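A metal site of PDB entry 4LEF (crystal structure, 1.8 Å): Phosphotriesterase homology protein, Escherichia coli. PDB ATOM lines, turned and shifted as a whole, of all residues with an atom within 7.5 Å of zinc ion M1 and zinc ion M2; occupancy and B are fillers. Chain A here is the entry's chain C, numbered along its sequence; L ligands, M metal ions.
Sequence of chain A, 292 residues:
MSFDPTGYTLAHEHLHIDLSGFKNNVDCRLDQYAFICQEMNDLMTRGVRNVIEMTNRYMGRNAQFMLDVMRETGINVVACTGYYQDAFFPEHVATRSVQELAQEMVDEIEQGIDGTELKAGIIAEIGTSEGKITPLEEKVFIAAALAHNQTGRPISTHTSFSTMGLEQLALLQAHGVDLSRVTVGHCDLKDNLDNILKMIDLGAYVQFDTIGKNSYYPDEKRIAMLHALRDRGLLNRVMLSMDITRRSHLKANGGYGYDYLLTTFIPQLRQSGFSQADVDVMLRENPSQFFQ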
ATOM      1  N   HIS A  12      26.154  -8.999  15.223  1.00  0.00           N
ATOM      2  CA  HIS A  12      26.196  -8.551  16.608  1.00  0.00           C
ATOM      3  C   HIS A  12      27.506  -7.860  16.897  1.00  0.00           C
ATOM      4  O   HIS A  12      28.525  -8.518  17.104  1.00  0.00           O
ATOM      5  CB  HIS A  12      26.000  -9.740  17.580  1.00  0.00           C
ATOM      6  CG  HIS A  12      25.983  -9.336  19.019  1.00  0.00           C
ATOM      7  ND1 HIS A  12      24.927  -9.644  19.861  1.00  0.00           N
ATOM      8  CD2 HIS A  12      26.892  -8.692  19.786  1.00  0.00           C
ATOM      9  CE1 HIS A  12      25.184  -9.182  21.070  1.00  0.00           C
ATOM     10  NE2 HIS A  12      26.372  -8.602  21.050  1.00  0.00           N
ATOM     11  N   GLU A  13      27.476  -6.532  16.899  1.00  0.00           N
ATOM     12  CA  GLU A  13      28.682  -5.735  17.117  1.00  0.00           C
ATOM     13  C   GLU A  13      28.368  -4.517  17.977  1.00  0.00           C
ATOM     14  O   GLU A  13      27.208  -4.158  18.167  1.00  0.00           O
ATOM     15  CB  GLU A  13      29.261  -5.240  15.780  1.00  0.00           C
ATOM     16  CG  GLU A  13      29.725  -6.345  14.853  1.00  0.00           C
ATOM     17  CD  GLU A  13      30.771  -7.230  15.468  1.00  0.00           C
ATOM     18  OE1 GLU A  13      31.455  -6.762  16.401  1.00  0.00           O
ATOM     19  OE2 GLU A  13      30.897  -8.396  15.016  1.00  0.00           O
ATOM     20  N   HIS A  14      29.412  -3.897  18.516  1.00  0.00           N
ATOM     21  CA  HIS A  14      29.261  -2.616  19.189  1.00  0.00           C
ATOM     22  C   HIS A  14      30.209  -1.649  18.495  1.00  0.00           C
ATOM     23  O   HIS A  14      31.321  -2.046  18.136  1.00  0.00           O
ATOM     24  CB  HIS A  14      29.587  -2.751  20.665  1.00  0.00           C
ATOM     25  CG  HIS A  14      28.689  -3.735  21.365  1.00  0.00           C
ATOM     26  ND1 HIS A  14      27.445  -3.379  21.849  1.00  0.00           N
ATOM     27  CD2 HIS A  14      28.821  -5.061  21.587  1.00  0.00           C
ATOM     28  CE1 HIS A  14      26.860  -4.451  22.361  1.00  0.00           C
ATOM     29  NE2 HIS A  14      27.666  -5.484  22.217  1.00  0.00           N
ATOM     30  N   ILE A  17      30.101   1.608  22.955  1.00  0.00           N
ATOM     31  CA  ILE A  17      29.480   1.042  24.148  1.00  0.00           C
ATOM     32  C   ILE A  17      30.301   1.510  25.333  1.00  0.00           C
ATOM     33  O   ILE A  17      31.506   1.693  25.205  1.00  0.00           O
ATOM     34  CB  ILE A  17      29.432  -0.492  24.065  1.00  0.00           C
ATOM     35  CG1 ILE A  17      28.932  -1.112  25.394  1.00  0.00           C
ATOM     36  CG2 ILE A  17      30.804  -1.055  23.660  1.00  0.00           C
ATOM     37  CD1 ILE A  17      28.643  -2.599  25.287  1.00  0.00           C
ATOM     38  N   GLU A  53      24.172  -3.032  15.350  1.00  0.00           N
ATOM     39  CA  GLU A  53      24.804  -2.510  16.552  1.00  0.00           C
ATOM     40  C   GLU A  53      23.933  -2.814  17.768  1.00  0.00           C
ATOM     41  O   GLU A  53      22.736  -2.521  17.785  1.00  0.00           O
ATOM     42  CB  GLU A  53      25.051  -1.002  16.387  1.00  0.00           C
ATOM     43  CG  GLU A  53      26.333  -0.504  17.040  1.00  0.00           C
ATOM     44  CD  GLU A  53      26.160  -0.189  18.518  1.00  0.00           C
ATOM     45  OE1 GLU A  53      25.006  -0.263  19.003  1.00  0.00           O
ATOM     46  OE2 GLU A  53      27.165   0.124  19.181  1.00  0.00           O
ATOM     47  N   MET A  54      24.537  -3.423  18.787  1.00  0.00           N
ATOM     48  CA  MET A  54      23.830  -4.024  19.907  1.00  0.00           C
ATOM     49  C   MET A  54      23.831  -3.209  21.205  1.00  0.00           C
ATOM     50  O   MET A  54      23.447  -3.725  22.262  1.00  0.00           O
ATOM     51  CB  MET A  54      24.441  -5.407  20.193  1.00  0.00           C
ATOM     52  CG  MET A  54      24.377  -6.397  19.008  1.00  0.00           C
ATOM     53  SD  MET A  54      22.764  -7.213  18.849  1.00  0.00           S
ATOM     54  CE  MET A  54      21.950  -6.173  17.643  1.00  0.00           C
ATOM     55  N   THR A  55      24.255  -1.946  21.130  1.00  0.00           N
ATOM     56  CA  THR A  55      24.323  -1.122  22.338  1.00  0.00           C
ATOM     57  C   THR A  55      23.009  -0.381  22.548  1.00  0.00           C
ATOM     58  O   THR A  55      22.716   0.551  21.806  1.00  0.00           O
ATOM     59  CB  THR A  55      25.455  -0.086  22.235  1.00  0.00           C
ATOM     60  OG1 THR A  55      26.643  -0.708  21.736  1.00  0.00           O
ATOM     61  CG2 THR A  55      25.755   0.525  23.611  1.00  0.00           C
ATOM     62  N   MET A  59      23.487   0.992  27.994  1.00  0.00           N
ATOM     63  CA  MET A  59      24.811   0.391  27.801  1.00  0.00           C
ATOM     64  C   MET A  59      25.793   1.430  27.239  1.00  0.00           C
ATOM     65  O   MET A  59      26.946   1.113  26.911  1.00  0.00           O
ATOM     66  CB  MET A  59      24.758  -0.796  26.831  1.00  0.00           C
ATOM     67  CG  MET A  59      23.846  -1.960  27.259  1.00  0.00           C
ATOM     68  SD  MET A  59      23.517  -3.135  25.902  1.00  0.00           S
ATOM     69  CE  MET A  59      25.107  -3.969  25.704  1.00  0.00           C
ATOM     70  N   TYR A  84      19.412  -4.242  28.811  1.00  0.00           N
ATOM     71  CA  TYR A  84      20.472  -5.235  28.657  1.00  0.00           C
ATOM     72  C   TYR A  84      20.271  -6.507  29.511  1.00  0.00           C
ATOM     73  O   TYR A  84      19.822  -7.533  28.994  1.00  0.00           O
ATOM     74  CB  TYR A  84      21.825  -4.548  28.933  1.00  0.00           C
ATOM     75  CG  TYR A  84      23.069  -5.378  28.736  1.00  0.00           C
ATOM     76  CD1 TYR A  84      23.121  -6.423  27.820  1.00  0.00           C
ATOM     77  CD2 TYR A  84      24.210  -5.112  29.498  1.00  0.00           C
ATOM     78  CE1 TYR A  84      24.295  -7.182  27.655  1.00  0.00           C
ATOM     79  CE2 TYR A  84      25.369  -5.855  29.354  1.00  0.00           C
ATOM     80  CZ  TYR A  84      25.411  -6.879  28.429  1.00  0.00           C
ATOM     81  OH  TYR A  84      26.581  -7.599  28.332  1.00  0.00           O
ATOM     82  N   GLN A  85      20.625  -6.454  30.788  1.00  0.00           N
ATOM     83  CA  GLN A  85      20.455  -7.606  31.668  1.00  0.00           C
ATOM     84  C   GLN A  85      20.414  -7.122  33.106  1.00  0.00           C
ATOM     85  O   GLN A  85      20.718  -5.966  33.383  1.00  0.00           O
ATOM     86  CB  GLN A  85      21.560  -8.656  31.450  1.00  0.00           C
ATOM     87  CG  GLN A  85      22.997  -8.134  31.587  1.00  0.00           C
ATOM     88  CD  GLN A  85      24.028  -9.251  31.623  1.00  0.00           C
ATOM     89  OE1 GLN A  85      23.978 -10.119  32.502  1.00  0.00           O
ATOM     90  NE2 GLN A  85      24.958  -9.258  30.661  1.00  0.00           N
ATOM     91  N   GLU A 125      20.492  -5.551  22.567  1.00  0.00           N
ATOM     92  CA  GLU A 125      20.569  -6.981  22.834  1.00  0.00           C
ATOM     93  C   GLU A 125      19.876  -7.168  24.163  1.00  0.00           C
ATOM     94  O   GLU A 125      20.288  -6.599  25.160  1.00  0.00           O
ATOM     95  CB  GLU A 125      22.020  -7.508  22.871  1.00  0.00           C
ATOM     96  CG  GLU A 125      23.039  -6.760  23.738  1.00  0.00           C
ATOM     97  CD  GLU A 125      24.357  -7.512  23.785  1.00  0.00           C
ATOM     98  OE1 GLU A 125      24.347  -8.674  24.238  1.00  0.00           O
ATOM     99  OE2 GLU A 125      25.402  -6.962  23.385  1.00  0.00           O
ATOM    100  N   ILE A 126      18.750  -7.870  24.151  1.00  0.00           N
ATOM    101  CA  ILE A 126      18.011  -8.047  25.392  1.00  0.00           C
ATOM    102  C   ILE A 126      18.420  -9.351  26.038  1.00  0.00           C
ATOM    103  O   ILE A 126      18.366 -10.414  25.429  1.00  0.00           O
ATOM    104  CB  ILE A 126      16.489  -7.911  25.170  1.00  0.00           C
ATOM    105  CG1 ILE A 126      15.989  -8.972  24.216  1.00  0.00           C
ATOM    106  CG2 ILE A 126      16.147  -6.509  24.636  1.00  0.00           C
ATOM    107  CD1 ILE A 126      14.475  -9.152  24.249  1.00  0.00           C
ATOM    108  N   GLY A 127      18.870  -9.266  27.285  1.00  0.00           N
ATOM    109  CA  GLY A 127      19.557 -10.397  27.866  1.00  0.00           C
ATOM    110  C   GLY A 127      18.972 -11.019  29.107  1.00  0.00           C
ATOM    111  O   GLY A 127      18.137 -10.431  29.796  1.00  0.00           O
ATOM    112  N   THR A 157      18.810 -11.398  21.078  1.00  0.00           N
ATOM    113  CA  THR A 157      18.981 -11.570  22.520  1.00  0.00           C
ATOM    114  C   THR A 157      20.438 -11.733  22.942  1.00  0.00           C
ATOM    115  O   THR A 157      21.321 -11.938  22.113  1.00  0.00           O
ATOM    116  CB  THR A 157      18.226 -12.780  23.051  1.00  0.00           C
ATOM    117  OG1 THR A 157      18.961 -13.971  22.722  1.00  0.00           O
ATOM    118  CG2 THR A 157      16.843 -12.857  22.455  1.00  0.00           C
ATOM    119  N   HIS A 158      20.653 -11.613  24.238  1.00  0.00           N
ATOM    120  CA  HIS A 158      21.913 -11.896  24.872  1.00  0.00           C
ATOM    121  C   HIS A 158      21.708 -13.130  25.742  1.00  0.00           C
ATOM    122  O   HIS A 158      20.801 -13.153  26.589  1.00  0.00           O
ATOM    123  CB  HIS A 158      22.340 -10.717  25.752  1.00  0.00           C
ATOM    124  CG  HIS A 158      23.344 -11.067  26.804  1.00  0.00           C
ATOM    125  ND1 HIS A 158      24.687 -10.773  26.679  1.00  0.00           N
ATOM    126  CD2 HIS A 158      23.207 -11.643  28.028  1.00  0.00           C
ATOM    127  CE1 HIS A 158      25.334 -11.194  27.748  1.00  0.00           C
ATOM    128  NE2 HIS A 158      24.460 -11.722  28.594  1.00  0.00           N
ATOM    129  N   THR A 159      22.531 -14.166  25.559  1.00  0.00           N
ATOM    130  CA  THR A 159      22.597 -15.220  26.570  1.00  0.00           C
ATOM    131  C   THR A 159      23.904 -15.129  27.361  1.00  0.00           C
ATOM    132  O   THR A 159      24.954 -14.790  26.822  1.00  0.00           O
ATOM    133  CB  THR A 159      22.411 -16.633  25.990  1.00  0.00           C
ATOM    134  OG1 THR A 159      23.450 -16.910  25.051  1.00  0.00           O
ATOM    135  CG2 THR A 159      21.048 -16.754  25.297  1.00  0.00           C
ATOM    136  N   SER A 160      23.808 -15.369  28.662  1.00  0.00           N
ATOM    137  CA  SER A 160      24.995 -15.347  29.513  1.00  0.00           C
ATOM    138  C   SER A 160      25.564 -16.760  29.590  1.00  0.00           C
ATOM    139  O   SER A 160      24.890 -17.678  30.052  1.00  0.00           O
ATOM    140  CB  SER A 160      24.645 -14.818  30.905  1.00  0.00           C
ATOM    141  OG  SER A 160      24.163 -13.479  30.819  1.00  0.00           O
ATOM    142  N   GLY A 185      21.602 -14.617  20.794  1.00  0.00           N
ATOM    143  CA  GLY A 185      23.012 -14.235  20.840  1.00  0.00           C
ATOM    144  C   GLY A 185      23.884 -15.098  21.737  1.00  0.00           C
ATOM    145  O   GLY A 185      23.402 -15.716  22.688  1.00  0.00           O
ATOM    146  N   HIS A 186      25.176 -15.131  21.412  1.00  0.00           N
ATOM    147  CA  HIS A 186      26.196 -15.786  22.227  1.00  0.00           C
ATOM    148  C   HIS A 186      25.956 -17.286  22.405  1.00  0.00           C
ATOM    149  O   HIS A 186      26.095 -17.832  23.508  1.00  0.00           O
ATOM    150  CB  HIS A 186      26.328 -15.130  23.623  1.00  0.00           C
ATOM    151  CG  HIS A 186      26.345 -13.622  23.603  1.00  0.00           C
ATOM    152  ND1 HIS A 186      26.932 -12.876  22.601  1.00  0.00           N
ATOM    153  CD2 HIS A 186      25.845 -12.719  24.499  1.00  0.00           C
ATOM    154  CE1 HIS A 186      26.794 -11.590  22.875  1.00  0.00           C
ATOM    155  NE2 HIS A 186      26.141 -11.470  24.018  1.00  0.00           N
ATOM    156  N   ASP A 209      28.596 -15.395  17.750  1.00  0.00           N
ATOM    157  CA  ASP A 209      28.988 -13.998  17.652  1.00  0.00           C
ATOM    158  C   ASP A 209      30.134 -13.659  18.593  1.00  0.00           C
ATOM    159  O   ASP A 209      30.411 -12.491  18.847  1.00  0.00           O
ATOM    160  CB  ASP A 209      27.775 -13.080  17.880  1.00  0.00           C
ATOM    161  CG  ASP A 209      27.021 -13.445  19.146  1.00  0.00           C
ATOM    162  OD1 ASP A 209      27.685 -13.933  20.084  1.00  0.00           O
ATOM    163  OD2 ASP A 209      25.783 -13.250  19.191  1.00  0.00           O
ATOM    164  N   THR A 210      30.838 -14.665  19.105  1.00  0.00           N
ATOM    165  CA  THR A 210      32.006 -14.378  19.938  1.00  0.00           C
ATOM    166  C   THR A 210      33.271 -14.969  19.344  1.00  0.00           C
ATOM    167  O   THR A 210      34.184 -15.374  20.071  1.00  0.00           O
ATOM    168  CB  THR A 210      31.818 -14.814  21.404  1.00  0.00           C
ATOM    169  OG1 THR A 210      31.636 -16.231  21.473  1.00  0.00           O
ATOM    170  CG2 THR A 210      30.601 -14.116  22.046  1.00  0.00           C
ATOM    171  N   LYS A 213      36.990 -14.708  20.701  1.00  0.00           N
ATOM    172  CA  LYS A 213      37.044 -14.659  22.172  1.00  0.00           C
ATOM    173  C   LYS A 213      37.458 -16.024  22.694  1.00  0.00           C
ATOM    174  O   LYS A 213      36.637 -16.764  23.244  1.00  0.00           O
ATOM    175  CB  LYS A 213      35.721 -14.186  22.775  1.00  0.00           C
ATOM    176  CG  LYS A 213      35.244 -12.885  22.117  1.00  0.00           C
ATOM    177  CD  LYS A 213      34.233 -12.110  22.942  1.00  0.00           C
ATOM    178  CE  LYS A 213      33.960 -10.761  22.267  1.00  0.00           C
ATOM    179  NZ  LYS A 213      33.276  -9.767  23.146  1.00  0.00           N
ATOM    180  N   ASP A 243      31.393  -9.544  17.982  1.00  0.00           N
ATOM    181  CA  ASP A 243      30.951  -8.876  19.228  1.00  0.00           C
ATOM    182  C   ASP A 243      32.095  -8.066  19.839  1.00  0.00           C
ATOM    183  O   ASP A 243      32.427  -8.233  21.011  1.00  0.00           O
ATOM    184  CB  ASP A 243      30.383  -9.887  20.248  1.00  0.00           C
ATOM    185  CG  ASP A 243      29.801  -9.217  21.480  1.00  0.00           C
ATOM    186  OD1 ASP A 243      29.291  -8.080  21.375  1.00  0.00           O
ATOM    187  OD2 ASP A 243      29.874  -9.836  22.569  1.00  0.00           O
ATOM    188  N   ILE A 244      32.700  -7.201  19.046  1.00  0.00           N
ATOM    189  CA  ILE A 244      33.699  -6.280  19.589  1.00  0.00           C
ATOM    190  C   ILE A 244      33.091  -5.419  20.696  1.00  0.00           C
ATOM    191  O   ILE A 244      32.061  -4.782  20.493  1.00  0.00           O
ATOM    192  CB  ILE A 244      34.222  -5.353  18.505  1.00  0.00           C
ATOM    193  CG1 ILE A 244      34.814  -6.169  17.362  1.00  0.00           C
ATOM    194  CG2 ILE A 244      35.188  -4.339  19.089  1.00  0.00           C
ATOM    195  CD1 ILE A 244      36.002  -7.069  17.762  1.00  0.00           C
ATOM    196  N   THR A 245      33.710  -5.411  21.867  1.00  0.00           N
ATOM    197  CA  THR A 245      33.141  -4.708  23.024  1.00  0.00           C
ATOM    198  C   THR A 245      34.173  -3.874  23.743  1.00  0.00           C
ATOM    199  O   THR A 245      33.812  -3.091  24.632  1.00  0.00           O
ATOM    200  CB  THR A 245      32.597  -5.702  24.073  1.00  0.00           C
ATOM    201  OG1 THR A 245      33.606  -6.656  24.411  1.00  0.00           O
ATOM    202  CG2 THR A 245      31.348  -6.403  23.566  1.00  0.00           C
HETATM  203  P1  LIG L   1      28.172  -8.360  25.385  1.00  0.00           P
HETATM  204  O1  LIG L   1      27.921  -8.599  23.929  1.00  0.00           O
HETATM  205  O2  LIG L   1      28.408  -6.908  25.744  1.00  0.00           O
HETATM  206  O3  LIG L   1      26.951  -8.834  26.170  1.00  0.00           O
HETATM  207  O4  LIG L   1      29.375  -9.172  25.742  1.00  0.00           O
HETATM  208 ZN    ZN M   1      25.671  -9.849  25.077  1.00  0.00          ZN
HETATM  209 ZN    ZN M   2      27.199  -7.460  22.530  1.00  0.00          ZN
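A ring nitrogen (NE2) of His 158 lies within hydrogen-bond range of the side-chain hydroxyl (OG) of Ser 160, 2.9 Å away.
NE2 of Gln 85 lies within hydrogen-bond range of OH of Tyr 84, at 3.3 Å.
The backbone carbonyl oxygen (O) of Tyr 84 lies within hydrogen-bond range of the backbone NH (N) of Gly 127 (2.6 Å).
The side-chain carboxylate (OD2) of Asp 243 is in salt-bridge range of the side-chain amino group (NZ) of Lys 213, at 3.5 Å.
O of Asp 209 sits close to N of Asp 243.
N of Glu 125 sits close to O of Met 54 (3.5 Å).
The backbone NH (N) of Asp 243 lies within hydrogen-bond range of the side-chain carboxylate (OE1) of Glu 13.
The side-chain carboxylate (OD1) of Asp 209 lies within hydrogen-bond range of a ring nitrogen (ND1) of His 186 (2.8 Å).
Tyr 84 touches zinc ion M1 (CE1 to ZN, 3.96 Å).
Of the 25 residues printed, 4 come within 4 Å of zinc ion M1.
Along chain A the residues within 4 Å of zinc ion M1 span positions 84 to 186.
Four residues have an atom within 4 Å of zinc ion M2: His 12, His 14, Glu 125 and Asp 243.
Zinc ion M1 is bound by OE1 of Glu 125 (2.0 Å), O3 of the ligand (2.0 Å), NE2 of His 186 (2.0 Å) and ND1 of His 158 (2.1 Å).
Zinc ion M1 has four donor atoms within binding distance.
Slightly farther from zinc ion M1 lies an oxygen (O1) of the ligand (2.8 Å).
Zinc ion M2 is bound by an oxygen (O1) of the ligand (1.9 Å), a ring nitrogen (NE2) of His 12 (2.0 Å), the side-chain carboxylate (OE2) of Glu 125 (2.1 Å), a ring nitrogen (NE2) of His 14 (2.1 Å) and the side-chain carboxylate (OD1) of Asp 243 (2.5 Å).
Zinc ion M2 has five donor atoms within binding distance.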
